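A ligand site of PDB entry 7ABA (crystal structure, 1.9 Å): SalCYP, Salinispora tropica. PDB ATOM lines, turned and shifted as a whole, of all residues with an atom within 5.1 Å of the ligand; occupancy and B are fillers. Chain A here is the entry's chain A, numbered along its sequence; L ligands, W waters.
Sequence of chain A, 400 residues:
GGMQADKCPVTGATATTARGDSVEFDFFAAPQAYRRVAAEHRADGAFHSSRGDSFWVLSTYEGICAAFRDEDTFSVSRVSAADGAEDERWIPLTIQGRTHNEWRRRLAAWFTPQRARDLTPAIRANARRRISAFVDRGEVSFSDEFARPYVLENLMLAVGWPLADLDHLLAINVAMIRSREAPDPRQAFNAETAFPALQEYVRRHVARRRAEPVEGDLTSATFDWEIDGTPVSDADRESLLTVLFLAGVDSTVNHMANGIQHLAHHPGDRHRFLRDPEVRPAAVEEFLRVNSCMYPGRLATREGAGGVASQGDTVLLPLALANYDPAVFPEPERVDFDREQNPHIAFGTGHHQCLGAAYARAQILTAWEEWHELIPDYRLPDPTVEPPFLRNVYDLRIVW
Phe 68 touches the ligand (CE1 to O2, 3.6 Å). O of Pro 92 touches O4 of the ligand, at 3.6 Å. CA of Leu 93 touches O4 of the ligand, 3.3 Å away. Phe 111 touches the ligand (CE1 to C26, 3.4 Å). Leu 155 touches the ligand. Leu 244 touches the ligand (CD2 to C31, 3.9 Å). Ala 247 touches the ligand. Gly 248 touches the ligand (CA to C22, 3.7 Å). Ser 251 touches the ligand. Thr 252 touches the ligand. CD2 of His 255 touches C19 of the ligand, 3.5 Å away. Leu 288 touches the ligand. Met 294 touches the ligand. Pro 296 touches the ligand. Leu 319 touches the ligand. Ala 346 touches the ligand (O to C17, 3.4 Å). CE1 of Phe 347 touches C15 of the ligand, at 3.5 Å. Gly 348 touches the ligand. CD2 of Leu 355 touches C31 of the ligand, 3.7 Å away. Gly 356 touches the ligand (CA to C22, 3.7 Å). Ala 360 touches the ligand. Hydrophobic or aromatic side chains within 4 Å of the ligand: Phe 68, Pro 92, Leu 93, His 100, Phe 111, Leu 155, Leu 244, Ala 247, His 255, Leu 288, Met 294, Pro 296, Leu 319, Phe 347, His 352, Leu 355 and Ala 360. Of the 32 residues printed, 26 come within 4 Å of the ligand. Along chain A the residues within 4 Å of the ligand span positions 68 to 360. The nearest printed residue that does not touch the ligand is Ile 364 (4.04 Å).
The backbone NH (N) of Cys 354 lies within hydrogen-bond range of the backbone carbonyl oxygen (O) of Phe 347, at 2.9 Å. N of Gly 356 lies close to SG of Cys 354, 3.2 Å away. NE2 of His 100 lies within hydrogen-bond range of ND1 of His 352 (3.3 Å). The guanidinium group (NH1) of Arg 104 sits at hydrogen-bond distance from the backbone carbonyl oxygen (O) of His 351 (3.5 Å). The guanidinium group (NH1) of Arg 104 sits at hydrogen-bond distance from the backbone carbonyl oxygen (O) of Gln 353 (2.8 Å). N of Leu 319 sits at hydrogen-bond distance from O of Met 294 (2.9 Å).
An iron atom (FE1) of the ligand is bound by the side-chain sulfur (SG) of Cys 354 (2.4 Å). O3 of the ligand lies within hydrogen-bond range of NE2 of His 100, at 2.7 Å. The guanidinium group of Arg 104 is in salt-bridge range of an oxygen (O3) of the ligand. ND1 of His 352 lies within hydrogen-bond range of O4 of the ligand, at 2.8 Å. O2 of the ligand lies within salt-bridge range of NH2 of Arg 298 (2.9 Å).
Water W4 lies within hydrogen-bond range of an oxygen (O2) of the ligand (2.8 Å) and the backbone NH (N) of Gln 353 (3.4 Å). Water W2 bridges O of Leu 93 (3.0 Å) and O1 of the ligand (3.0 Å). Water W5 bridges OG1 of Thr 252 (2.9 Å) and O of Ala 247 (3.0 Å). Water W3 lies within hydrogen-bond range of O of Ala 346 (2.8 Å) and NE2 of His 255 (3.1 Å).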
ATOM      1  N   PHE A  68       5.305 -22.264   7.351  1.00  0.00           N
ATOM      2  CA  PHE A  68       6.659 -22.497   6.869  1.00  0.00           C
ATOM      3  C   PHE A  68       7.096 -23.933   7.095  1.00  0.00           C
ATOM      4  O   PHE A  68       7.881 -24.477   6.305  1.00  0.00           O
ATOM      5  CB  PHE A  68       7.657 -21.565   7.559  1.00  0.00           C
ATOM      6  CG  PHE A  68       7.832 -20.217   6.890  1.00  0.00           C
ATOM      7  CD1 PHE A  68       8.335 -20.113   5.608  1.00  0.00           C
ATOM      8  CD2 PHE A  68       7.550 -19.060   7.593  1.00  0.00           C
ATOM      9  CE1 PHE A  68       8.530 -18.863   5.021  1.00  0.00           C
ATOM     10  CE2 PHE A  68       7.736 -17.805   7.015  1.00  0.00           C
ATOM     11  CZ  PHE A  68       8.227 -17.707   5.723  1.00  0.00           C
ATOM     12  N   PRO A  92      17.146 -23.418  -5.330  1.00  0.00           N
ATOM     13  CA  PRO A  92      16.313 -24.482  -4.743  1.00  0.00           C
ATOM     14  C   PRO A  92      14.957 -23.996  -4.227  1.00  0.00           C
ATOM     15  O   PRO A  92      14.235 -24.764  -3.588  1.00  0.00           O
ATOM     16  CB  PRO A  92      17.187 -24.968  -3.575  1.00  0.00           C
ATOM     17  CG  PRO A  92      17.896 -23.716  -3.119  1.00  0.00           C
ATOM     18  CD  PRO A  92      18.036 -22.814  -4.326  1.00  0.00           C
ATOM     19  N   LEU A  93      14.594 -22.750  -4.552  1.00  0.00           N
ATOM     20  CA  LEU A  93      13.423 -22.104  -3.957  1.00  0.00           C
ATOM     21  C   LEU A  93      12.126 -22.868  -4.223  1.00  0.00           C
ATOM     22  O   LEU A  93      11.237 -22.913  -3.363  1.00  0.00           O
ATOM     23  CB  LEU A  93      13.286 -20.672  -4.465  1.00  0.00           C
ATOM     24  CG  LEU A  93      14.094 -19.607  -3.724  1.00  0.00           C
ATOM     25  CD1 LEU A  93      14.149 -18.323  -4.552  1.00  0.00           C
ATOM     26  CD2 LEU A  93      13.464 -19.330  -2.356  1.00  0.00           C
ATOM     27  N   HIS A 100      14.767 -31.399  -2.699  1.00  0.00           N
ATOM     28  CA  HIS A 100      15.217 -30.151  -2.100  1.00  0.00           C
ATOM     29  C   HIS A 100      16.297 -30.405  -1.050  1.00  0.00           C
ATOM     30  O   HIS A 100      17.303 -29.686  -1.001  1.00  0.00           O
ATOM     31  CB  HIS A 100      14.037 -29.412  -1.474  1.00  0.00           C
ATOM     32  CG  HIS A 100      14.443 -28.167  -0.747  1.00  0.00           C
ATOM     33  ND1 HIS A 100      14.581 -28.128   0.622  1.00  0.00           N
ATOM     34  CD2 HIS A 100      14.781 -26.939  -1.196  1.00  0.00           C
ATOM     35  CE1 HIS A 100      14.977 -26.924   0.992  1.00  0.00           C
ATOM     36  NE2 HIS A 100      15.101 -26.177  -0.099  1.00  0.00           N
ATOM     37  N   ARG A 104      20.149 -28.883  -0.816  1.00  0.00           N
ATOM     38  CA  ARG A 104      20.684 -28.239   0.382  1.00  0.00           C
ATOM     39  C   ARG A 104      21.903 -28.983   0.925  1.00  0.00           C
ATOM     40  O   ARG A 104      22.830 -28.353   1.434  1.00  0.00           O
ATOM     41  CB  ARG A 104      19.605 -28.124   1.459  1.00  0.00           C
ATOM     42  CG  ARG A 104      18.442 -27.167   1.127  1.00  0.00           C
ATOM     43  CD  ARG A 104      18.879 -25.717   0.939  1.00  0.00           C
ATOM     44  NE  ARG A 104      19.402 -25.151   2.185  1.00  0.00           N
ATOM     45  CZ  ARG A 104      18.830 -24.210   2.921  1.00  0.00           C
ATOM     46  NH1 ARG A 104      17.677 -23.648   2.561  1.00  0.00           N
ATOM     47  NH2 ARG A 104      19.420 -23.801   4.036  1.00  0.00           N
ATOM     48  N   PHE A 111      28.214 -22.593   2.702  1.00  0.00           N
ATOM     49  CA  PHE A 111      27.507 -21.554   3.454  1.00  0.00           C
ATOM     50  C   PHE A 111      27.329 -21.920   4.925  1.00  0.00           C
ATOM     51  O   PHE A 111      26.378 -21.475   5.570  1.00  0.00           O
ATOM     52  CB  PHE A 111      26.145 -21.280   2.815  1.00  0.00           C
ATOM     53  CG  PHE A 111      26.264 -20.687   1.438  1.00  0.00           C
ATOM     54  CD1 PHE A 111      26.498 -19.338   1.274  1.00  0.00           C
ATOM     55  CD2 PHE A 111      26.205 -21.501   0.315  1.00  0.00           C
ATOM     56  CE1 PHE A 111      26.647 -18.811   0.016  1.00  0.00           C
ATOM     57  CE2 PHE A 111      26.344 -20.970  -0.944  1.00  0.00           C
ATOM     58  CZ  PHE A 111      26.565 -19.625  -1.088  1.00  0.00           C
ATOM     59  N   LEU A 155      29.497 -11.677  -1.815  1.00  0.00           N
ATOM     60  CA  LEU A 155      28.792 -12.767  -2.489  1.00  0.00           C
ATOM     61  C   LEU A 155      29.672 -13.397  -3.570  1.00  0.00           C
ATOM     62  O   LEU A 155      29.765 -14.620  -3.679  1.00  0.00           O
ATOM     63  CB  LEU A 155      27.488 -12.254  -3.091  1.00  0.00           C
ATOM     64  CG  LEU A 155      26.613 -13.289  -3.797  1.00  0.00           C
ATOM     65  CD1 LEU A 155      26.101 -14.335  -2.819  1.00  0.00           C
ATOM     66  CD2 LEU A 155      25.458 -12.609  -4.523  1.00  0.00           C
ATOM     67  N   VAL A 243      19.672 -17.761  -8.888  1.00  0.00           N
ATOM     68  CA  VAL A 243      19.025 -17.570  -7.592  1.00  0.00           C
ATOM     69  C   VAL A 243      20.002 -16.988  -6.573  1.00  0.00           C
ATOM     70  O   VAL A 243      19.647 -16.086  -5.795  1.00  0.00           O
ATOM     71  CB  VAL A 243      18.408 -18.901  -7.111  1.00  0.00           C
ATOM     72  CG1 VAL A 243      17.992 -18.829  -5.644  1.00  0.00           C
ATOM     73  CG2 VAL A 243      17.231 -19.250  -7.980  1.00  0.00           C
ATOM     74  N   LEU A 244      21.243 -17.497  -6.547  1.00  0.00           N
ATOM     75  CA  LEU A 244      22.223 -16.977  -5.602  1.00  0.00           C
ATOM     76  C   LEU A 244      22.473 -15.489  -5.831  1.00  0.00           C
ATOM     77  O   LEU A 244      22.571 -14.717  -4.873  1.00  0.00           O
ATOM     78  CB  LEU A 244      23.529 -17.761  -5.706  1.00  0.00           C
ATOM     79  CG  LEU A 244      23.438 -19.199  -5.195  1.00  0.00           C
ATOM     80  CD1 LEU A 244      24.703 -19.968  -5.543  1.00  0.00           C
ATOM     81  CD2 LEU A 244      23.180 -19.241  -3.701  1.00  0.00           C
ATOM     82  N   ALA A 247      19.176 -13.550  -4.761  1.00  0.00           N
ATOM     83  CA  ALA A 247      18.874 -13.668  -3.350  1.00  0.00           C
ATOM     84  C   ALA A 247      19.945 -13.058  -2.442  1.00  0.00           C
ATOM     85  O   ALA A 247      19.638 -12.714  -1.302  1.00  0.00           O
ATOM     86  CB  ALA A 247      18.714 -15.146  -2.979  1.00  0.00           C
ATOM     87  N   GLY A 248      21.166 -12.916  -2.928  1.00  0.00           N
ATOM     88  CA  GLY A 248      22.308 -12.716  -2.074  1.00  0.00           C
ATOM     89  C   GLY A 248      22.781 -11.286  -1.857  1.00  0.00           C
ATOM     90  O   GLY A 248      23.832 -11.095  -1.257  1.00  0.00           O
ATOM     91  N   SER A 251      18.543  -7.994   0.266  1.00  0.00           N
ATOM     92  CA  SER A 251      18.084  -8.107   1.650  1.00  0.00           C
ATOM     93  C   SER A 251      19.184  -7.738   2.635  1.00  0.00           C
ATOM     94  O   SER A 251      18.923  -7.078   3.653  1.00  0.00           O
ATOM     95  CB  SER A 251      17.570  -9.520   1.912  1.00  0.00           C
ATOM     96  OG  SER A 251      16.288  -9.692   1.343  1.00  0.00           O
ATOM     97  N   THR A 252      20.420  -8.154   2.360  1.00  0.00           N
ATOM     98  CA  THR A 252      21.539  -7.814   3.238  1.00  0.00           C
ATOM     99  C   THR A 252      21.800  -6.310   3.229  1.00  0.00           C
ATOM    100  O   THR A 252      21.960  -5.693   4.286  1.00  0.00           O
ATOM    101  CB  THR A 252      22.802  -8.579   2.799  1.00  0.00           C
ATOM    102  OG1 THR A 252      22.511  -9.980   2.745  1.00  0.00           O
ATOM    103  CG2 THR A 252      23.974  -8.337   3.769  1.00  0.00           C
ATOM    104  N   HIS A 255      18.961  -4.425   5.095  1.00  0.00           N
ATOM    105  CA  HIS A 255      19.103  -4.553   6.543  1.00  0.00           C
ATOM    106  C   HIS A 255      20.250  -3.685   7.064  1.00  0.00           C
ATOM    107  O   HIS A 255      20.120  -3.041   8.108  1.00  0.00           O
ATOM    108  CB  HIS A 255      19.301  -6.019   6.935  1.00  0.00           C
ATOM    109  CG  HIS A 255      18.023  -6.744   7.179  1.00  0.00           C
ATOM    110  ND1 HIS A 255      17.220  -6.468   8.259  1.00  0.00           N
ATOM    111  CD2 HIS A 255      17.399  -7.737   6.498  1.00  0.00           C
ATOM    112  CE1 HIS A 255      16.153  -7.258   8.235  1.00  0.00           C
ATOM    113  NE2 HIS A 255      16.242  -8.038   7.174  1.00  0.00           N
ATOM    114  N   LEU A 288      17.504  -7.267  12.649  1.00  0.00           N
ATOM    115  CA  LEU A 288      16.956  -8.227  11.706  1.00  0.00           C
ATOM    116  C   LEU A 288      15.465  -8.446  11.959  1.00  0.00           C
ATOM    117  O   LEU A 288      14.663  -8.508  11.012  1.00  0.00           O
ATOM    118  CB  LEU A 288      17.728  -9.550  11.781  1.00  0.00           C
ATOM    119  CG  LEU A 288      19.102  -9.604  11.100  1.00  0.00           C
ATOM    120  CD1 LEU A 288      19.898 -10.813  11.577  1.00  0.00           C
ATOM    121  CD2 LEU A 288      18.941  -9.647   9.590  1.00  0.00           C
ATOM    122  N   MET A 294      10.211  -9.207   4.010  1.00  0.00           N
ATOM    123  CA  MET A 294       9.851 -10.193   3.005  1.00  0.00           C
ATOM    124  C   MET A 294       8.493 -10.804   3.324  1.00  0.00           C
ATOM    125  O   MET A 294       8.072 -10.887   4.486  1.00  0.00           O
ATOM    126  CB  MET A 294      10.902 -11.295   2.926  1.00  0.00           C
ATOM    127  CG  MET A 294      12.201 -10.840   2.299  1.00  0.00           C
ATOM    128  SD  MET A 294      13.522 -12.057   2.473  1.00  0.00           S
ATOM    129  CE  MET A 294      12.905 -13.425   1.489  1.00  0.00           C
ATOM    130  N   PRO A 296       7.263 -14.174   1.876  1.00  0.00           N
ATOM    131  CA  PRO A 296       7.271 -15.413   1.102  1.00  0.00           C
ATOM    132  C   PRO A 296       5.862 -15.955   0.899  1.00  0.00           C
ATOM    133  O   PRO A 296       5.026 -15.908   1.811  1.00  0.00           O
ATOM    134  CB  PRO A 296       8.119 -16.361   1.945  1.00  0.00           C
ATOM    135  CG  PRO A 296       8.956 -15.480   2.797  1.00  0.00           C
ATOM    136  CD  PRO A 296       8.106 -14.288   3.085  1.00  0.00           C
ATOM    137  N   ARG A 298       3.180 -19.108  -0.431  1.00  0.00           N
ATOM    138  CA  ARG A 298       2.964 -20.541  -0.518  1.00  0.00           C
ATOM    139  C   ARG A 298       1.625 -20.797  -1.181  1.00  0.00           C
ATOM    140  O   ARG A 298       0.721 -19.962  -1.150  1.00  0.00           O
ATOM    141  CB  ARG A 298       2.988 -21.211   0.861  1.00  0.00           C
ATOM    142  CG  ARG A 298       4.313 -21.116   1.601  1.00  0.00           C
ATOM    143  CD  ARG A 298       5.417 -21.826   0.849  1.00  0.00           C
ATOM    144  NE  ARG A 298       6.635 -21.998   1.623  1.00  0.00           N
ATOM    145  CZ  ARG A 298       7.694 -21.190   1.585  1.00  0.00           C
ATOM    146  NH1 ARG A 298       7.711 -20.102   0.817  1.00  0.00           N
ATOM    147  NH2 ARG A 298       8.749 -21.484   2.326  1.00  0.00           N
ATOM    148  N   LEU A 319       7.015 -11.630   7.123  1.00  0.00           N
ATOM    149  CA  LEU A 319       7.903 -11.583   8.286  1.00  0.00           C
ATOM    150  C   LEU A 319       7.659 -10.332   9.111  1.00  0.00           C
ATOM    151  O   LEU A 319       7.912 -10.330  10.327  1.00  0.00           O
ATOM    152  CB  LEU A 319       9.355 -11.669   7.832  1.00  0.00           C
ATOM    153  CG  LEU A 319       9.699 -12.868   6.944  1.00  0.00           C
ATOM    154  CD1 LEU A 319      11.169 -12.886   6.604  1.00  0.00           C
ATOM    155  CD2 LEU A 319       9.317 -14.164   7.631  1.00  0.00           C
ATOM    156  N   ALA A 346      13.580 -13.754  10.804  1.00  0.00           N
ATOM    157  CA  ALA A 346      13.999 -12.887   9.700  1.00  0.00           C
ATOM    158  C   ALA A 346      14.537 -13.673   8.514  1.00  0.00           C
ATOM    159  O   ALA A 346      14.544 -13.152   7.393  1.00  0.00           O
ATOM    160  CB  ALA A 346      15.083 -11.910  10.198  1.00  0.00           C
ATOM    161  N   PHE A 347      15.000 -14.902   8.750  1.00  0.00           N
ATOM    162  CA  PHE A 347      15.528 -15.766   7.712  1.00  0.00           C
ATOM    163  C   PHE A 347      14.576 -16.901   7.367  1.00  0.00           C
ATOM    164  O   PHE A 347      14.979 -17.874   6.718  1.00  0.00           O
ATOM    165  CB  PHE A 347      16.880 -16.325   8.150  1.00  0.00           C
ATOM    166  CG  PHE A 347      17.954 -15.283   8.248  1.00  0.00           C
ATOM    167  CD1 PHE A 347      18.456 -14.679   7.115  1.00  0.00           C
ATOM    168  CD2 PHE A 347      18.449 -14.900   9.493  1.00  0.00           C
ATOM    169  CE1 PHE A 347      19.448 -13.713   7.209  1.00  0.00           C
ATOM    170  CE2 PHE A 347      19.428 -13.940   9.586  1.00  0.00           C
ATOM    171  CZ  PHE A 347      19.927 -13.346   8.444  1.00  0.00           C
ATOM    172  N   GLY A 348      13.313 -16.806   7.786  1.00  0.00           N
ATOM    173  CA  GLY A 348      12.366 -17.878   7.554  1.00  0.00           C
ATOM    174  C   GLY A 348      12.537 -19.020   8.546  1.00  0.00           C
ATOM    175  O   GLY A 348      13.259 -18.934   9.528  1.00  0.00           O
ATOM    176  N   HIS A 351      12.095 -25.920   5.878  1.00  0.00           N
ATOM    177  CA  HIS A 351      13.158 -26.451   5.015  1.00  0.00           C
ATOM    178  C   HIS A 351      13.834 -25.370   4.179  1.00  0.00           C
ATOM    179  O   HIS A 351      15.012 -25.497   3.871  1.00  0.00           O
ATOM    180  CB  HIS A 351      12.601 -27.516   4.071  1.00  0.00           C
ATOM    181  CG  HIS A 351      12.070 -28.719   4.784  1.00  0.00           C
ATOM    182  ND1 HIS A 351      12.826 -29.454   5.672  1.00  0.00           N
ATOM    183  CD2 HIS A 351      10.861 -29.325   4.735  1.00  0.00           C
ATOM    184  CE1 HIS A 351      12.102 -30.452   6.145  1.00  0.00           C
ATOM    185  NE2 HIS A 351      10.907 -30.398   5.585  1.00  0.00           N
ATOM    186  N   HIS A 352      13.114 -24.335   3.784  1.00  0.00           N
ATOM    187  CA  HIS A 352      13.659 -23.328   2.881  1.00  0.00           C
ATOM    188  C   HIS A 352      14.311 -22.169   3.617  1.00  0.00           C
ATOM    189  O   HIS A 352      14.652 -21.164   2.979  1.00  0.00           O
ATOM    190  CB  HIS A 352      12.555 -22.838   1.936  1.00  0.00           C
ATOM    191  CG  HIS A 352      12.118 -23.878   0.954  1.00  0.00           C
ATOM    192  ND1 HIS A 352      12.670 -23.974  -0.304  1.00  0.00           N
ATOM    193  CD2 HIS A 352      11.210 -24.872   1.038  1.00  0.00           C
ATOM    194  CE1 HIS A 352      12.114 -24.980  -0.952  1.00  0.00           C
ATOM    195  NE2 HIS A 352      11.231 -25.551  -0.157  1.00  0.00           N
ATOM    196  N   GLN A 353      14.506 -22.298   4.925  1.00  0.00           N
ATOM    197  CA  GLN A 353      15.174 -21.281   5.716  1.00  0.00           C
ATOM    198  C   GLN A 353      16.477 -20.853   5.042  1.00  0.00           C
ATOM    199  O   GLN A 353      17.218 -21.680   4.511  1.00  0.00           O
ATOM    200  CB  GLN A 353      15.465 -21.839   7.113  1.00  0.00           C
ATOM    201  CG  GLN A 353      16.055 -20.849   8.096  1.00  0.00           C
ATOM    202  CD  GLN A 353      16.347 -21.499   9.432  1.00  0.00           C
ATOM    203  OE1 GLN A 353      15.565 -22.311   9.923  1.00  0.00           O
ATOM    204  NE2 GLN A 353      17.487 -21.161  10.029  1.00  0.00           N
ATOM    205  N   CYS A 354      16.733 -19.550   5.064  1.00  0.00           N
ATOM    206  CA  CYS A 354      17.802 -18.944   4.272  1.00  0.00           C
ATOM    207  C   CYS A 354      19.116 -19.706   4.318  1.00  0.00           C
ATOM    208  O   CYS A 354      19.706 -19.916   5.387  1.00  0.00           O
ATOM    209  CB  CYS A 354      18.027 -17.520   4.764  1.00  0.00           C
ATOM    210  SG  CYS A 354      19.330 -16.657   3.893  1.00  0.00           S
ATOM    211  N   LEU A 355      19.618 -20.056   3.134  1.00  0.00           N
ATOM    212  CA  LEU A 355      20.928 -20.674   2.973  1.00  0.00           C
ATOM    213  C   LEU A 355      22.052 -19.738   3.426  1.00  0.00           C
ATOM    214  O   LEU A 355      23.081 -20.207   3.914  1.00  0.00           O
ATOM    215  CB  LEU A 355      21.116 -21.056   1.501  1.00  0.00           C
ATOM    216  CG  LEU A 355      22.453 -21.586   1.009  1.00  0.00           C
ATOM    217  CD1 LEU A 355      22.671 -23.006   1.518  1.00  0.00           C
ATOM    218  CD2 LEU A 355      22.523 -21.538  -0.523  1.00  0.00           C
ATOM    219  N   GLY A 356      21.859 -18.436   3.262  1.00  0.00           N
ATOM    220  CA  GLY A 356      22.929 -17.486   3.521  1.00  0.00           C
ATOM    221  C   GLY A 356      22.870 -16.769   4.852  1.00  0.00           C
ATOM    222  O   GLY A 356      23.502 -15.720   5.005  1.00  0.00           O
ATOM    223  N   TYR A 359      26.179 -16.117   6.668  1.00  0.00           N
ATOM    224  CA  TYR A 359      26.979 -15.177   5.882  1.00  0.00           C
ATOM    225  C   TYR A 359      26.415 -13.760   5.965  1.00  0.00           C
ATOM    226  O   TYR A 359      27.162 -12.782   6.079  1.00  0.00           O
ATOM    227  CB  TYR A 359      27.049 -15.640   4.434  1.00  0.00           C
ATOM    228  CG  TYR A 359      28.233 -15.121   3.656  1.00  0.00           C
ATOM    229  CD1 TYR A 359      29.499 -15.163   4.187  1.00  0.00           C
ATOM    230  CD2 TYR A 359      28.078 -14.607   2.369  1.00  0.00           C
ATOM    231  CE1 TYR A 359      30.592 -14.697   3.491  1.00  0.00           C
ATOM    232  CE2 TYR A 359      29.179 -14.124   1.662  1.00  0.00           C
ATOM    233  CZ  TYR A 359      30.437 -14.181   2.224  1.00  0.00           C
ATOM    234  OH  TYR A 359      31.557 -13.725   1.541  1.00  0.00           O
ATOM    235  N   ALA A 360      25.089 -13.625   5.855  1.00  0.00           N
ATOM    236  CA  ALA A 360      24.487 -12.298   5.966  1.00  0.00           C
ATOM    237  C   ALA A 360      24.751 -11.683   7.338  1.00  0.00           C
ATOM    238  O   ALA A 360      25.103 -10.506   7.448  1.00  0.00           O
ATOM    239  CB  ALA A 360      22.979 -12.387   5.681  1.00  0.00           C
ATOM    240  N   GLN A 363      28.256 -10.359   7.441  1.00  0.00           N
ATOM    241  CA  GLN A 363      28.442  -9.144   6.665  1.00  0.00           C
ATOM    242  C   GLN A 363      27.907  -7.918   7.382  1.00  0.00           C
ATOM    243  O   GLN A 363      28.536  -6.851   7.372  1.00  0.00           O
ATOM    244  CB  GLN A 363      27.770  -9.285   5.298  1.00  0.00           C
ATOM    245  CG  GLN A 363      28.442 -10.281   4.390  1.00  0.00           C
ATOM    246  CD  GLN A 363      27.766 -10.343   3.045  1.00  0.00           C
ATOM    247  OE1 GLN A 363      27.894  -9.421   2.238  1.00  0.00           O
ATOM    248  NE2 GLN A 363      27.023 -11.421   2.801  1.00  0.00           N
ATOM    249  N   ILE A 364      26.717  -8.041   7.978  1.00  0.00           N
ATOM    250  CA  ILE A 364      26.090  -6.923   8.643  1.00  0.00           C
ATOM    251  C   ILE A 364      26.907  -6.518   9.866  1.00  0.00           C
ATOM    252  O   ILE A 364      27.272  -5.353  10.028  1.00  0.00           O
ATOM    253  CB  ILE A 364      24.644  -7.277   9.033  1.00  0.00           C
ATOM    254  CG1 ILE A 364      23.811  -7.508   7.761  1.00  0.00           C
ATOM    255  CG2 ILE A 364      24.017  -6.174   9.891  1.00  0.00           C
ATOM    256  CD1 ILE A 364      22.504  -8.218   8.042  1.00  0.00           C
HETATM  257 FE1  LIG L   1      18.261 -15.585   2.053  1.00  0.00          FE
HETATM  258  C1  LIG L   1      15.963 -18.045   1.337  1.00  0.00           C
HETATM  259  C2  LIG L   1      15.915 -13.997   3.967  1.00  0.00           C
HETATM  260  C3  LIG L   1      20.566 -13.157   2.792  1.00  0.00           C
HETATM  261  C4  LIG L   1      20.505 -16.965  -0.159  1.00  0.00           C
HETATM  262  N1  LIG L   1      16.292 -15.940   2.525  1.00  0.00           N
HETATM  263  C5  LIG L   1      15.559 -17.062   2.196  1.00  0.00           C
HETATM  264  C6  LIG L   1      14.289 -17.015   2.891  1.00  0.00           C
HETATM  265  C7  LIG L   1      14.287 -15.879   3.627  1.00  0.00           C
HETATM  266  C8  LIG L   1      15.536 -15.194   3.406  1.00  0.00           C
HETATM  267  C9  LIG L   1      13.160 -15.360   4.549  1.00  0.00           C
HETATM  268  C10 LIG L   1      13.178 -18.096   2.796  1.00  0.00           C
HETATM  269  C11 LIG L   1      12.241 -17.801   1.626  1.00  0.00           C
HETATM  270  C12 LIG L   1      11.117 -18.798   1.571  1.00  0.00           C
HETATM  271  O1  LIG L   1      10.347 -18.758   0.575  1.00  0.00           O
HETATM  272  O2  LIG L   1      11.006 -19.651   2.493  1.00  0.00           O
HETATM  273  N2  LIG L   1      18.238 -13.879   3.140  1.00  0.00           N
HETATM  274  C13 LIG L   1      17.158 -13.418   3.869  1.00  0.00           C
HETATM  275  C14 LIG L   1      17.572 -12.194   4.529  1.00  0.00           C
HETATM  276  C15 LIG L   1      18.862 -11.975   4.228  1.00  0.00           C
HETATM  277  C16 LIG L   1      19.305 -13.030   3.338  1.00  0.00           C
HETATM  278  C17 LIG L   1      16.638 -11.374   5.446  1.00  0.00           C
HETATM  279  C18 LIG L   1      19.787 -10.814   4.631  1.00  0.00           C
HETATM  280  C19 LIG L   1      19.680 -10.337   6.076  1.00  0.00           C
HETATM  281  N3  LIG L   1      20.180 -15.118   1.395  1.00  0.00           N
HETATM  282  C20 LIG L   1      20.978 -14.123   1.912  1.00  0.00           C
HETATM  283  C21 LIG L   1      22.299 -14.266   1.338  1.00  0.00           C
HETATM  284  C22 LIG L   1      22.284 -15.348   0.536  1.00  0.00           C
HETATM  285  C23 LIG L   1      20.945 -15.886   0.557  1.00  0.00           C
HETATM  286  C24 LIG L   1      23.499 -13.347   1.696  1.00  0.00           C
HETATM  287  C25 LIG L   1      23.429 -15.943  -0.317  1.00  0.00           C
HETATM  288  C26 LIG L   1      24.717 -16.095   0.508  1.00  0.00           C
HETATM  289  N4  LIG L   1      18.227 -17.217   0.815  1.00  0.00           N
HETATM  290  C27 LIG L   1      19.279 -17.580  -0.026  1.00  0.00           C
HETATM  291  C28 LIG L   1      18.893 -18.749  -0.781  1.00  0.00           C
HETATM  292  C29 LIG L   1      17.489 -19.090  -0.311  1.00  0.00           C
HETATM  293  C30 LIG L   1      17.157 -18.092   0.669  1.00  0.00           C
HETATM  294  C31 LIG L   1      19.751 -19.486  -1.831  1.00  0.00           C
HETATM  295  C32 LIG L   1      16.592 -20.248  -0.793  1.00  0.00           C
HETATM  296  C33 LIG L   1      16.782 -21.434   0.143  1.00  0.00           C
HETATM  297  C34 LIG L   1      15.845 -22.566  -0.232  1.00  0.00           C
HETATM  298  O3  LIG L   1      16.087 -23.709   0.229  1.00  0.00           O
HETATM  299  O4  LIG L   1      14.869 -22.313  -0.967  1.00  0.00           O
HETATM  300  O   HOH W   1      10.321 -16.670  -0.884  1.00  0.00           O
HETATM  301  O   HOH W   2      10.304 -20.578  -1.800  1.00  0.00           O
HETATM  302  O   HOH W   3      14.182 -10.347   7.366  1.00  0.00           O
HETATM  303  O   HOH W   4      11.843 -20.209   5.066  1.00  0.00           O
HETATM  304  O   HOH W   5      20.679 -10.752   0.681  1.00  0.00           O
